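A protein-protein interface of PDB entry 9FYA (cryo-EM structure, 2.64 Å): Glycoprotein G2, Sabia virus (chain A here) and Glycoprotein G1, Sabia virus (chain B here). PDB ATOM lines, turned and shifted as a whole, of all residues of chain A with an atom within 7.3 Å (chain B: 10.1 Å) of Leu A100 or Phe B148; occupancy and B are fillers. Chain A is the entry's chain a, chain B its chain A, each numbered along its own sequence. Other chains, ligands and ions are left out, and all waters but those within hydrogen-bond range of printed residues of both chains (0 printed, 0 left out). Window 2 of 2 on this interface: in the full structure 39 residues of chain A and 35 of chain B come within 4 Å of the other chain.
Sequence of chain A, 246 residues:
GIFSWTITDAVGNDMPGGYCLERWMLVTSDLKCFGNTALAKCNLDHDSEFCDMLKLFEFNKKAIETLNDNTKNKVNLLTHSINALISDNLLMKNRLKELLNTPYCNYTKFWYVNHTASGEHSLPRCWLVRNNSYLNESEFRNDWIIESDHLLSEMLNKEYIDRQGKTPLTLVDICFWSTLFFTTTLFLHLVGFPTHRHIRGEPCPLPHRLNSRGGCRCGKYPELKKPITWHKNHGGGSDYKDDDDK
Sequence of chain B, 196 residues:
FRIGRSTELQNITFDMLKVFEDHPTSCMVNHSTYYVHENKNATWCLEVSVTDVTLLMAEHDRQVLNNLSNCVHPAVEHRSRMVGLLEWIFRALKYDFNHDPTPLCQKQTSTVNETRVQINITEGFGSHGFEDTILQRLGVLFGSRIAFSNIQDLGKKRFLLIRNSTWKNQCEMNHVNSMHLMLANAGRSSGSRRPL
Arg A95 touches Gly B139 (CD to O, 3.5 Å). Arg A95 touches Gly B143. Gly B139 touches Leu A99. Leu A99 touches Gly B143. Ser B144 touches Leu A99. CE1 of Phe B148 touches CB of Leu A99, at 3.8 Å. Leu A100 touches Phe B148. Asn A101 touches Arg B145.
Of the 20 printed residues of chain B, 6 touch a printed residue of chain A. Printed residues of chain B that touch a printed residue of chain A: Gly B139, Val B140, Gly B143, Ser B144, Arg B145 and Phe B148. Among the printed residues, no Asp or Glu carboxylate lies within 4 Å of a Lys or Arg side-chain nitrogen of the other chain.
NE of Arg A95 lies within hydrogen-bond range of O of Val B140. O of Leu A99 is in hydrogen-bond range of NE of Arg B145.
Printed residues of chain B within 4 Å of Leu A100: Phe B148 (3.9 Å). Of chain A, only Leu A99 (3.8 Å) and Leu A100 (3.9 Å) come within 4 Å of Phe B148. No residue of chain B comes within 4 Å of Thr A102. Of the printed residues of chain A, Arg B145 touches Leu A99 (2.7 Å) and Asn A101 (3.5 Å). Printed residues of chain A within 4 Å of Val B140: Arg A95. Of the printed residues of chain B, Arg A95 touches Gly B139 (3.5 Å), Val B140 (2.8 Å) and Gly B143 (3.3 Å). Of the printed residues of chain A, Ser B144 touches Leu A99. The nearest residue of chain A that does not touch Phe B148 is Leu A96 (6.2 Å).
The guanidinium group (NH1) of Arg A95 is in salt-bridge range of the side-chain carboxylate (OE1) of Glu A98 (2.7 Å). O of His B31 lies within hydrogen-bond range of OG of Ser B144. ND1 of His B31 lies within hydrogen-bond range of N of Arg B145. OH of Tyr B34 sits at hydrogen-bond distance from OG of Ser B144. The side-chain hydroxyl (OG) of Ser B144 sits at hydrogen-bond distance from the backbone NH (N) of Ile B146 (3.3 Å).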
ATOM      1  N   LYS A  93     -16.400  12.793  10.485  1.00  0.00           N
ATOM      2  CA  LYS A  93     -16.385  11.974   9.281  1.00  0.00           C
ATOM      3  C   LYS A  93     -17.599  12.256   8.417  1.00  0.00           C
ATOM      4  O   LYS A  93     -17.484  12.367   7.193  1.00  0.00           O
ATOM      5  CB  LYS A  93     -16.326  10.490   9.634  1.00  0.00           C
ATOM      6  CG  LYS A  93     -14.996  10.035  10.177  1.00  0.00           C
ATOM      7  CD  LYS A  93     -14.996   8.550  10.488  1.00  0.00           C
ATOM      8  CE  LYS A  93     -15.057   8.292  11.979  1.00  0.00           C
ATOM      9  NZ  LYS A  93     -14.675   6.894  12.302  1.00  0.00           N
ATOM     10  N   ASN A  94     -18.776  12.364   9.032  1.00  0.00           N
ATOM     11  CA  ASN A  94     -19.971  12.653   8.250  1.00  0.00           C
ATOM     12  C   ASN A  94     -19.895  14.034   7.607  1.00  0.00           C
ATOM     13  O   ASN A  94     -20.317  14.214   6.460  1.00  0.00           O
ATOM     14  CB  ASN A  94     -21.214  12.501   9.118  1.00  0.00           C
ATOM     15  CG  ASN A  94     -21.518  11.059   9.425  1.00  0.00           C
ATOM     16  OD1 ASN A  94     -21.685  10.255   8.516  1.00  0.00           O
ATOM     17  ND2 ASN A  94     -21.592  10.720  10.701  1.00  0.00           N
ATOM     18  N   ARG A  95     -19.362  15.024   8.326  1.00  0.00           N
ATOM     19  CA  ARG A  95     -19.214  16.352   7.736  1.00  0.00           C
ATOM     20  C   ARG A  95     -18.247  16.337   6.557  1.00  0.00           C
ATOM     21  O   ARG A  95     -18.505  16.969   5.527  1.00  0.00           O
ATOM     22  CB  ARG A  95     -18.751  17.361   8.785  1.00  0.00           C
ATOM     23  CG  ARG A  95     -18.572  18.756   8.210  1.00  0.00           C
ATOM     24  CD  ARG A  95     -19.893  19.378   7.781  1.00  0.00           C
ATOM     25  NE  ARG A  95     -20.605  20.011   8.884  1.00  0.00           N
ATOM     26  CZ  ARG A  95     -21.866  20.412   8.836  1.00  0.00           C
ATOM     27  NH1 ARG A  95     -22.605  20.239   7.757  1.00  0.00           N
ATOM     28  NH2 ARG A  95     -22.391  21.028   9.886  1.00  0.00           N
ATOM     29  N   LEU A  96     -17.125  15.627   6.689  1.00  0.00           N
ATOM     30  CA  LEU A  96     -16.172  15.546   5.585  1.00  0.00           C
ATOM     31  C   LEU A  96     -16.758  14.793   4.399  1.00  0.00           C
ATOM     32  O   LEU A  96     -16.479  15.133   3.245  1.00  0.00           O
ATOM     33  CB  LEU A  96     -14.876  14.886   6.051  1.00  0.00           C
ATOM     34  CG  LEU A  96     -13.999  15.761   6.944  1.00  0.00           C
ATOM     35  CD1 LEU A  96     -12.881  14.951   7.570  1.00  0.00           C
ATOM     36  CD2 LEU A  96     -13.458  16.959   6.185  1.00  0.00           C
ATOM     37  N   LYS A  97     -17.568  13.769   4.661  1.00  0.00           N
ATOM     38  CA  LYS A  97     -18.264  13.072   3.586  1.00  0.00           C
ATOM     39  C   LYS A  97     -19.230  14.014   2.873  1.00  0.00           C
ATOM     40  O   LYS A  97     -19.336  13.991   1.644  1.00  0.00           O
ATOM     41  CB  LYS A  97     -18.980  11.845   4.160  1.00  0.00           C
ATOM     42  CG  LYS A  97     -17.995  10.775   4.633  1.00  0.00           C
ATOM     43  CD  LYS A  97     -18.632   9.506   5.185  1.00  0.00           C
ATOM     44  CE  LYS A  97     -19.191   8.593   4.133  1.00  0.00           C
ATOM     45  NZ  LYS A  97     -18.106   7.827   3.470  1.00  0.00           N
ATOM     46  N   GLU A  98     -19.939  14.855   3.633  1.00  0.00           N
ATOM     47  CA  GLU A  98     -20.852  15.824   3.030  1.00  0.00           C
ATOM     48  C   GLU A  98     -20.107  16.854   2.187  1.00  0.00           C
ATOM     49  O   GLU A  98     -20.574  17.238   1.109  1.00  0.00           O
ATOM     50  CB  GLU A  98     -21.678  16.521   4.109  1.00  0.00           C
ATOM     51  CG  GLU A  98     -22.261  17.851   3.668  1.00  0.00           C
ATOM     52  CD  GLU A  98     -23.033  18.549   4.759  1.00  0.00           C
ATOM     53  OE1 GLU A  98     -22.747  18.302   5.944  1.00  0.00           O
ATOM     54  OE2 GLU A  98     -23.927  19.353   4.434  1.00  0.00           O
ATOM     55  N   LEU A  99     -18.950  17.322   2.663  1.00  0.00           N
ATOM     56  CA  LEU A  99     -18.202  18.337   1.927  1.00  0.00           C
ATOM     57  C   LEU A  99     -17.690  17.807   0.595  1.00  0.00           C
ATOM     58  O   LEU A  99     -17.466  18.588  -0.335  1.00  0.00           O
ATOM     59  CB  LEU A  99     -17.035  18.856   2.766  1.00  0.00           C
ATOM     60  CG  LEU A  99     -17.360  19.596   4.060  1.00  0.00           C
ATOM     61  CD1 LEU A  99     -16.104  20.121   4.715  1.00  0.00           C
ATOM     62  CD2 LEU A  99     -18.306  20.732   3.757  1.00  0.00           C
ATOM     63  N   LEU A 100     -17.487  16.496   0.485  1.00  0.00           N
ATOM     64  CA  LEU A 100     -16.985  15.883  -0.733  1.00  0.00           C
ATOM     65  C   LEU A 100     -18.090  15.249  -1.567  1.00  0.00           C
ATOM     66  O   LEU A 100     -17.790  14.499  -2.500  1.00  0.00           O
ATOM     67  CB  LEU A 100     -15.925  14.836  -0.392  1.00  0.00           C
ATOM     68  CG  LEU A 100     -14.701  15.331   0.380  1.00  0.00           C
ATOM     69  CD1 LEU A 100     -14.010  14.175   1.076  1.00  0.00           C
ATOM     70  CD2 LEU A 100     -13.737  16.068  -0.526  1.00  0.00           C
ATOM     71  N   ASN A 101     -19.355  15.524  -1.247  1.00  0.00           N
ATOM     72  CA  ASN A 101     -20.542  15.020  -1.940  1.00  0.00           C
ATOM     73  C   ASN A 101     -20.728  13.511  -1.811  1.00  0.00           C
ATOM     74  O   ASN A 101     -21.620  12.949  -2.455  1.00  0.00           O
ATOM     75  CB  ASN A 101     -20.537  15.424  -3.418  1.00  0.00           C
ATOM     76  CG  ASN A 101     -20.620  16.927  -3.605  1.00  0.00           C
ATOM     77  OD1 ASN A 101     -21.461  17.588  -3.003  1.00  0.00           O
ATOM     78  ND2 ASN A 101     -19.743  17.472  -4.437  1.00  0.00           N
ATOM     79  N   THR A 102     -19.901  12.842  -1.015  1.00  0.00           N
ATOM     80  CA  THR A 102     -20.093  11.435  -0.691  1.00  0.00           C
ATOM     81  C   THR A 102     -21.317  11.263   0.213  1.00  0.00           C
ATOM     82  O   THR A 102     -21.626  12.157   1.003  1.00  0.00           O
ATOM     83  CB  THR A 102     -18.824  10.900  -0.016  1.00  0.00           C
ATOM     84  OG1 THR A 102     -17.795  10.752  -1.000  1.00  0.00           O
ATOM     85  CG2 THR A 102     -19.044   9.562   0.675  1.00  0.00           C
ATOM     86  N   PRO A 103     -22.069  10.165   0.073  1.00  0.00           N
ATOM     87  CA  PRO A 103     -23.223   9.942   0.956  1.00  0.00           C
ATOM     88  C   PRO A 103     -22.825  10.013   2.423  1.00  0.00           C
ATOM     89  O   PRO A 103     -21.842   9.409   2.846  1.00  0.00           O
ATOM     90  CB  PRO A 103     -23.683   8.533   0.579  1.00  0.00           C
ATOM     91  CG  PRO A 103     -23.246   8.348  -0.796  1.00  0.00           C
ATOM     92  CD  PRO A 103     -21.986   9.141  -0.982  1.00  0.00           C
ATOM     93  N   HIS B  31     -23.409  29.444   0.283  1.00  0.00           N
ATOM     94  CA  HIS B  31     -22.036  29.098   0.645  1.00  0.00           C
ATOM     95  C   HIS B  31     -21.215  30.277   1.150  1.00  0.00           C
ATOM     96  O   HIS B  31     -20.078  30.067   1.580  1.00  0.00           O
ATOM     97  CB  HIS B  31     -21.328  28.428  -0.532  1.00  0.00           C
ATOM     98  CG  HIS B  31     -21.842  27.055  -0.831  1.00  0.00           C
ATOM     99  ND1 HIS B  31     -21.971  26.085   0.140  1.00  0.00           N
ATOM    100  CD2 HIS B  31     -22.269  26.491  -1.984  1.00  0.00           C
ATOM    101  CE1 HIS B  31     -22.452  24.982  -0.404  1.00  0.00           C
ATOM    102  NE2 HIS B  31     -22.642  25.201  -1.691  1.00  0.00           N
ATOM    103  N   TYR B  34     -23.971  32.965   6.445  1.00  0.00           N
ATOM    104  CA  TYR B  34     -24.302  32.018   7.495  1.00  0.00           C
ATOM    105  C   TYR B  34     -24.951  32.821   8.609  1.00  0.00           C
ATOM    106  O   TYR B  34     -24.692  34.014   8.753  1.00  0.00           O
ATOM    107  CB  TYR B  34     -23.036  31.347   8.039  1.00  0.00           C
ATOM    108  CG  TYR B  34     -22.147  30.863   6.935  1.00  0.00           C
ATOM    109  CD1 TYR B  34     -22.499  29.817   6.106  1.00  0.00           C
ATOM    110  CD2 TYR B  34     -20.937  31.506   6.705  1.00  0.00           C
ATOM    111  CE1 TYR B  34     -21.665  29.432   5.077  1.00  0.00           C
ATOM    112  CE2 TYR B  34     -20.109  31.130   5.695  1.00  0.00           C
ATOM    113  CZ  TYR B  34     -20.468  30.096   4.885  1.00  0.00           C
ATOM    114  OH  TYR B  34     -19.611  29.743   3.879  1.00  0.00           O
ATOM    115  N   GLU B 131      -6.182  31.463   4.984  1.00  0.00           N
ATOM    116  CA  GLU B 131      -7.436  31.537   4.246  1.00  0.00           C
ATOM    117  C   GLU B 131      -8.052  30.157   4.086  1.00  0.00           C
ATOM    118  O   GLU B 131      -9.253  29.971   4.303  1.00  0.00           O
ATOM    119  CB  GLU B 131      -7.193  32.173   2.880  1.00  0.00           C
ATOM    120  CG  GLU B 131      -8.442  32.336   2.042  1.00  0.00           C
ATOM    121  CD  GLU B 131      -8.188  33.133   0.779  1.00  0.00           C
ATOM    122  OE1 GLU B 131      -7.033  33.545   0.563  1.00  0.00           O
ATOM    123  OE2 GLU B 131      -9.137  33.347   0.004  1.00  0.00           O
ATOM    124  N   ASP B 132      -7.238  29.179   3.697  1.00  0.00           N
ATOM    125  CA  ASP B 132      -7.721  27.815   3.542  1.00  0.00           C
ATOM    126  C   ASP B 132      -8.168  27.235   4.875  1.00  0.00           C
ATOM    127  O   ASP B 132      -9.163  26.508   4.939  1.00  0.00           O
ATOM    128  CB  ASP B 132      -6.632  26.960   2.904  1.00  0.00           C
ATOM    129  CG  ASP B 132      -6.167  27.519   1.576  1.00  0.00           C
ATOM    130  OD1 ASP B 132      -7.026  27.921   0.767  1.00  0.00           O
ATOM    131  OD2 ASP B 132      -4.943  27.572   1.345  1.00  0.00           O
ATOM    132  N   ILE B 134      -9.460  28.915   7.420  1.00  0.00           N
ATOM    133  CA  ILE B 134     -10.743  29.531   7.748  1.00  0.00           C
ATOM    134  C   ILE B 134     -11.859  28.988   6.864  1.00  0.00           C
ATOM    135  O   ILE B 134     -12.966  28.717   7.340  1.00  0.00           O
ATOM    136  CB  ILE B 134     -10.632  31.062   7.640  1.00  0.00           C
ATOM    137  CG1 ILE B 134      -9.726  31.613   8.740  1.00  0.00           C
ATOM    138  CG2 ILE B 134     -12.005  31.714   7.695  1.00  0.00           C
ATOM    139  CD1 ILE B 134     -10.265  31.431  10.122  1.00  0.00           C
ATOM    140  N   LEU B 135     -11.599  28.831   5.567  1.00  0.00           N
ATOM    141  CA  LEU B 135     -12.627  28.326   4.663  1.00  0.00           C
ATOM    142  C   LEU B 135     -13.000  26.887   4.989  1.00  0.00           C
ATOM    143  O   LEU B 135     -14.178  26.516   4.939  1.00  0.00           O
ATOM    144  CB  LEU B 135     -12.166  28.462   3.214  1.00  0.00           C
ATOM    145  CG  LEU B 135     -12.023  29.898   2.698  1.00  0.00           C
ATOM    146  CD1 LEU B 135     -11.759  29.919   1.204  1.00  0.00           C
ATOM    147  CD2 LEU B 135     -13.250  30.720   3.032  1.00  0.00           C
ATOM    148  N   GLN B 136     -12.016  26.055   5.330  1.00  0.00           N
ATOM    149  CA  GLN B 136     -12.343  24.697   5.742  1.00  0.00           C
ATOM    150  C   GLN B 136     -13.067  24.674   7.082  1.00  0.00           C
ATOM    151  O   GLN B 136     -13.915  23.804   7.304  1.00  0.00           O
ATOM    152  CB  GLN B 136     -11.078  23.849   5.780  1.00  0.00           C
ATOM    153  CG  GLN B 136     -10.542  23.527   4.404  1.00  0.00           C
ATOM    154  CD  GLN B 136      -9.088  23.130   4.420  1.00  0.00           C
ATOM    155  OE1 GLN B 136      -8.460  23.070   5.473  1.00  0.00           O
ATOM    156  NE2 GLN B 136      -8.536  22.871   3.246  1.00  0.00           N
ATOM    157  N   ARG B 137     -12.767  25.618   7.984  1.00  0.00           N
ATOM    158  CA  ARG B 137     -13.566  25.727   9.204  1.00  0.00           C
ATOM    159  C   ARG B 137     -15.004  26.095   8.890  1.00  0.00           C
ATOM    160  O   ARG B 137     -15.925  25.627   9.558  1.00  0.00           O
ATOM    161  CB  ARG B 137     -12.973  26.726  10.195  1.00  0.00           C
ATOM    162  CG  ARG B 137     -11.696  26.283  10.816  1.00  0.00           C
ATOM    163  CD  ARG B 137     -11.964  25.006  11.602  1.00  0.00           C
ATOM    164  NE  ARG B 137     -13.008  25.166  12.606  1.00  0.00           N
ATOM    165  CZ  ARG B 137     -13.544  24.162  13.287  1.00  0.00           C
ATOM    166  NH1 ARG B 137     -13.153  22.913  13.098  1.00  0.00           N
ATOM    167  NH2 ARG B 137     -14.497  24.418  14.180  1.00  0.00           N
ATOM    168  N   LEU B 138     -15.210  26.986   7.927  1.00  0.00           N
ATOM    169  CA  LEU B 138     -16.568  27.324   7.521  1.00  0.00           C
ATOM    170  C   LEU B 138     -17.282  26.105   6.962  1.00  0.00           C
ATOM    171  O   LEU B 138     -18.469  25.892   7.228  1.00  0.00           O
ATOM    172  CB  LEU B 138     -16.529  28.442   6.484  1.00  0.00           C
ATOM    173  CG  LEU B 138     -16.018  29.788   6.983  1.00  0.00           C
ATOM    174  CD1 LEU B 138     -16.397  30.846   6.006  1.00  0.00           C
ATOM    175  CD2 LEU B 138     -16.594  30.110   8.344  1.00  0.00           C
ATOM    176  N   GLY B 139     -16.567  25.287   6.194  1.00  0.00           N
ATOM    177  CA  GLY B 139     -17.144  24.043   5.714  1.00  0.00           C
ATOM    178  C   GLY B 139     -17.516  23.089   6.833  1.00  0.00           C
ATOM    179  O   GLY B 139     -18.563  22.445   6.791  1.00  0.00           O
ATOM    180  N   VAL B 140     -16.660  22.981   7.846  1.00  0.00           N
ATOM    181  CA  VAL B 140     -16.931  22.074   8.957  1.00  0.00           C
ATOM    182  C   VAL B 140     -18.083  22.594   9.812  1.00  0.00           C
ATOM    183  O   VAL B 140     -18.963  21.831  10.227  1.00  0.00           O
ATOM    184  CB  VAL B 140     -15.651  21.868   9.787  1.00  0.00           C
ATOM    185  CG1 VAL B 140     -15.961  21.207  11.117  1.00  0.00           C
ATOM    186  CG2 VAL B 140     -14.631  21.080   9.001  1.00  0.00           C
ATOM    187  N   GLY B 143     -21.312  23.515   6.983  1.00  0.00           N
ATOM    188  CA  GLY B 143     -21.483  22.655   5.831  1.00  0.00           C
ATOM    189  C   GLY B 143     -21.243  23.330   4.505  1.00  0.00           C
ATOM    190  O   GLY B 143     -21.724  22.848   3.479  1.00  0.00           O
ATOM    191  N   SER B 144     -20.506  24.434   4.499  1.00  0.00           N
ATOM    192  CA  SER B 144     -20.269  25.204   3.292  1.00  0.00           C
ATOM    193  C   SER B 144     -19.228  24.532   2.406  1.00  0.00           C
ATOM    194  O   SER B 144     -18.376  23.776   2.875  1.00  0.00           O
ATOM    195  CB  SER B 144     -19.813  26.615   3.658  1.00  0.00           C
ATOM    196  OG  SER B 144     -19.672  27.426   2.511  1.00  0.00           O
ATOM    197  N   ARG B 145     -19.306  24.807   1.106  1.00  0.00           N
ATOM    198  CA  ARG B 145     -18.323  24.314   0.152  1.00  0.00           C
ATOM    199  C   ARG B 145     -17.483  25.445  -0.437  1.00  0.00           C
ATOM    200  O   ARG B 145     -16.844  25.262  -1.475  1.00  0.00           O
ATOM    201  CB  ARG B 145     -18.999  23.486  -0.941  1.00  0.00           C
ATOM    202  CG  ARG B 145     -19.519  22.150  -0.419  1.00  0.00           C
ATOM    203  CD  ARG B 145     -19.975  21.209  -1.519  1.00  0.00           C
ATOM    204  NE  ARG B 145     -18.932  20.275  -1.924  1.00  0.00           N
ATOM    205  CZ  ARG B 145     -18.079  20.478  -2.918  1.00  0.00           C
ATOM    206  NH1 ARG B 145     -18.115  21.582  -3.646  1.00  0.00           N
ATOM    207  NH2 ARG B 145     -17.164  19.551  -3.187  1.00  0.00           N
ATOM    208  N   ILE B 146     -17.490  26.617   0.209  1.00  0.00           N
ATOM    209  CA  ILE B 146     -16.709  27.774  -0.227  1.00  0.00           C
ATOM    210  C   ILE B 146     -15.237  27.426  -0.412  1.00  0.00           C
ATOM    211  O   ILE B 146     -14.562  27.996  -1.275  1.00  0.00           O
ATOM    212  CB  ILE B 146     -16.903  28.948   0.767  1.00  0.00           C
ATOM    213  CG1 ILE B 146     -16.369  30.257   0.187  1.00  0.00           C
ATOM    214  CG2 ILE B 146     -16.258  28.660   2.113  1.00  0.00           C
ATOM    215  CD1 ILE B 146     -17.195  30.815  -0.932  1.00  0.00           C
ATOM    216  N   ALA B 147     -14.712  26.498   0.393  1.00  0.00           N
ATOM    217  CA  ALA B 147     -13.293  26.170   0.314  1.00  0.00           C
ATOM    218  C   ALA B 147     -12.954  25.438  -0.978  1.00  0.00           C
ATOM    219  O   ALA B 147     -11.826  25.540  -1.470  1.00  0.00           O
ATOM    220  CB  ALA B 147     -12.879  25.323   1.513  1.00  0.00           C
ATOM    221  N   PHE B 148     -13.906  24.696  -1.534  1.00  0.00           N
ATOM    222  CA  PHE B 148     -13.676  23.902  -2.738  1.00  0.00           C
ATOM    223  C   PHE B 148     -13.944  24.729  -3.989  1.00  0.00           C
ATOM    224  O   PHE B 148     -14.668  24.324  -4.892  1.00  0.00           O
ATOM    225  CB  PHE B 148     -14.569  22.669  -2.700  1.00  0.00           C
ATOM    226  CG  PHE B 148     -14.359  21.804  -1.495  1.00  0.00           C
ATOM    227  CD1 PHE B 148     -15.060  22.049  -0.328  1.00  0.00           C
ATOM    228  CD2 PHE B 148     -13.498  20.727  -1.530  1.00  0.00           C
ATOM    229  CE1 PHE B 148     -14.881  21.259   0.785  1.00  0.00           C
ATOM    230  CE2 PHE B 148     -13.329  19.924  -0.419  1.00  0.00           C
ATOM    231  CZ  PHE B 148     -14.015  20.196   0.739  1.00  0.00           C
ATOM    232  N   SER B 149     -13.326  25.905  -4.044  1.00  0.00           N
ATOM    233  CA  SER B 149     -13.497  26.837  -5.145  1.00  0.00           C
ATOM    234  C   SER B 149     -12.192  27.583  -5.365  1.00  0.00           C
ATOM    235  O   SER B 149     -11.310  27.592  -4.503  1.00  0.00           O
ATOM    236  CB  SER B 149     -14.638  27.824  -4.876  1.00  0.00           C
ATOM    237  OG  SER B 149     -15.887  27.163  -4.856  1.00  0.00           O
ATOM    238  N   ASN B 150     -12.070  28.193  -6.538  1.00  0.00           N
ATOM    239  CA  ASN B 150     -10.874  28.959  -6.872  1.00  0.00           C
ATOM    240  C   ASN B 150     -10.742  30.196  -5.982  1.00  0.00           C
ATOM    241  O   ASN B 150      -9.657  30.759  -5.841  1.00  0.00           O
ATOM    242  CB  ASN B 150     -10.895  29.371  -8.347  1.00  0.00           C
ATOM    243  CG  ASN B 150     -12.082  30.254  -8.695  1.00  0.00           C
ATOM    244  OD1 ASN B 150     -12.895  30.595  -7.838  1.00  0.00           O
ATOM    245  ND2 ASN B 150     -12.177  30.640  -9.963  1.00  0.00           N
ATOM    246  N   ARG B 158     -10.247  39.275   0.350  1.00  0.00           N
ATOM    247  CA  ARG B 158     -11.352  38.500   0.881  1.00  0.00           C
ATOM    248  C   ARG B 158     -11.355  38.598   2.396  1.00  0.00           C
ATOM    249  O   ARG B 158     -10.298  38.589   3.030  1.00  0.00           O
ATOM    250  CB  ARG B 158     -11.275  37.042   0.421  1.00  0.00           C
ATOM    251  CG  ARG B 158     -12.466  36.227   0.835  1.00  0.00           C
ATOM    252  CD  ARG B 158     -12.794  35.151  -0.169  1.00  0.00           C
ATOM    253  NE  ARG B 158     -11.718  34.192  -0.362  1.00  0.00           N
ATOM    254  CZ  ARG B 158     -11.843  33.076  -1.063  1.00  0.00           C
ATOM    255  NH1 ARG B 158     -12.987  32.745  -1.638  1.00  0.00           N
ATOM    256  NH2 ARG B 158     -10.789  32.277  -1.202  1.00  0.00           N
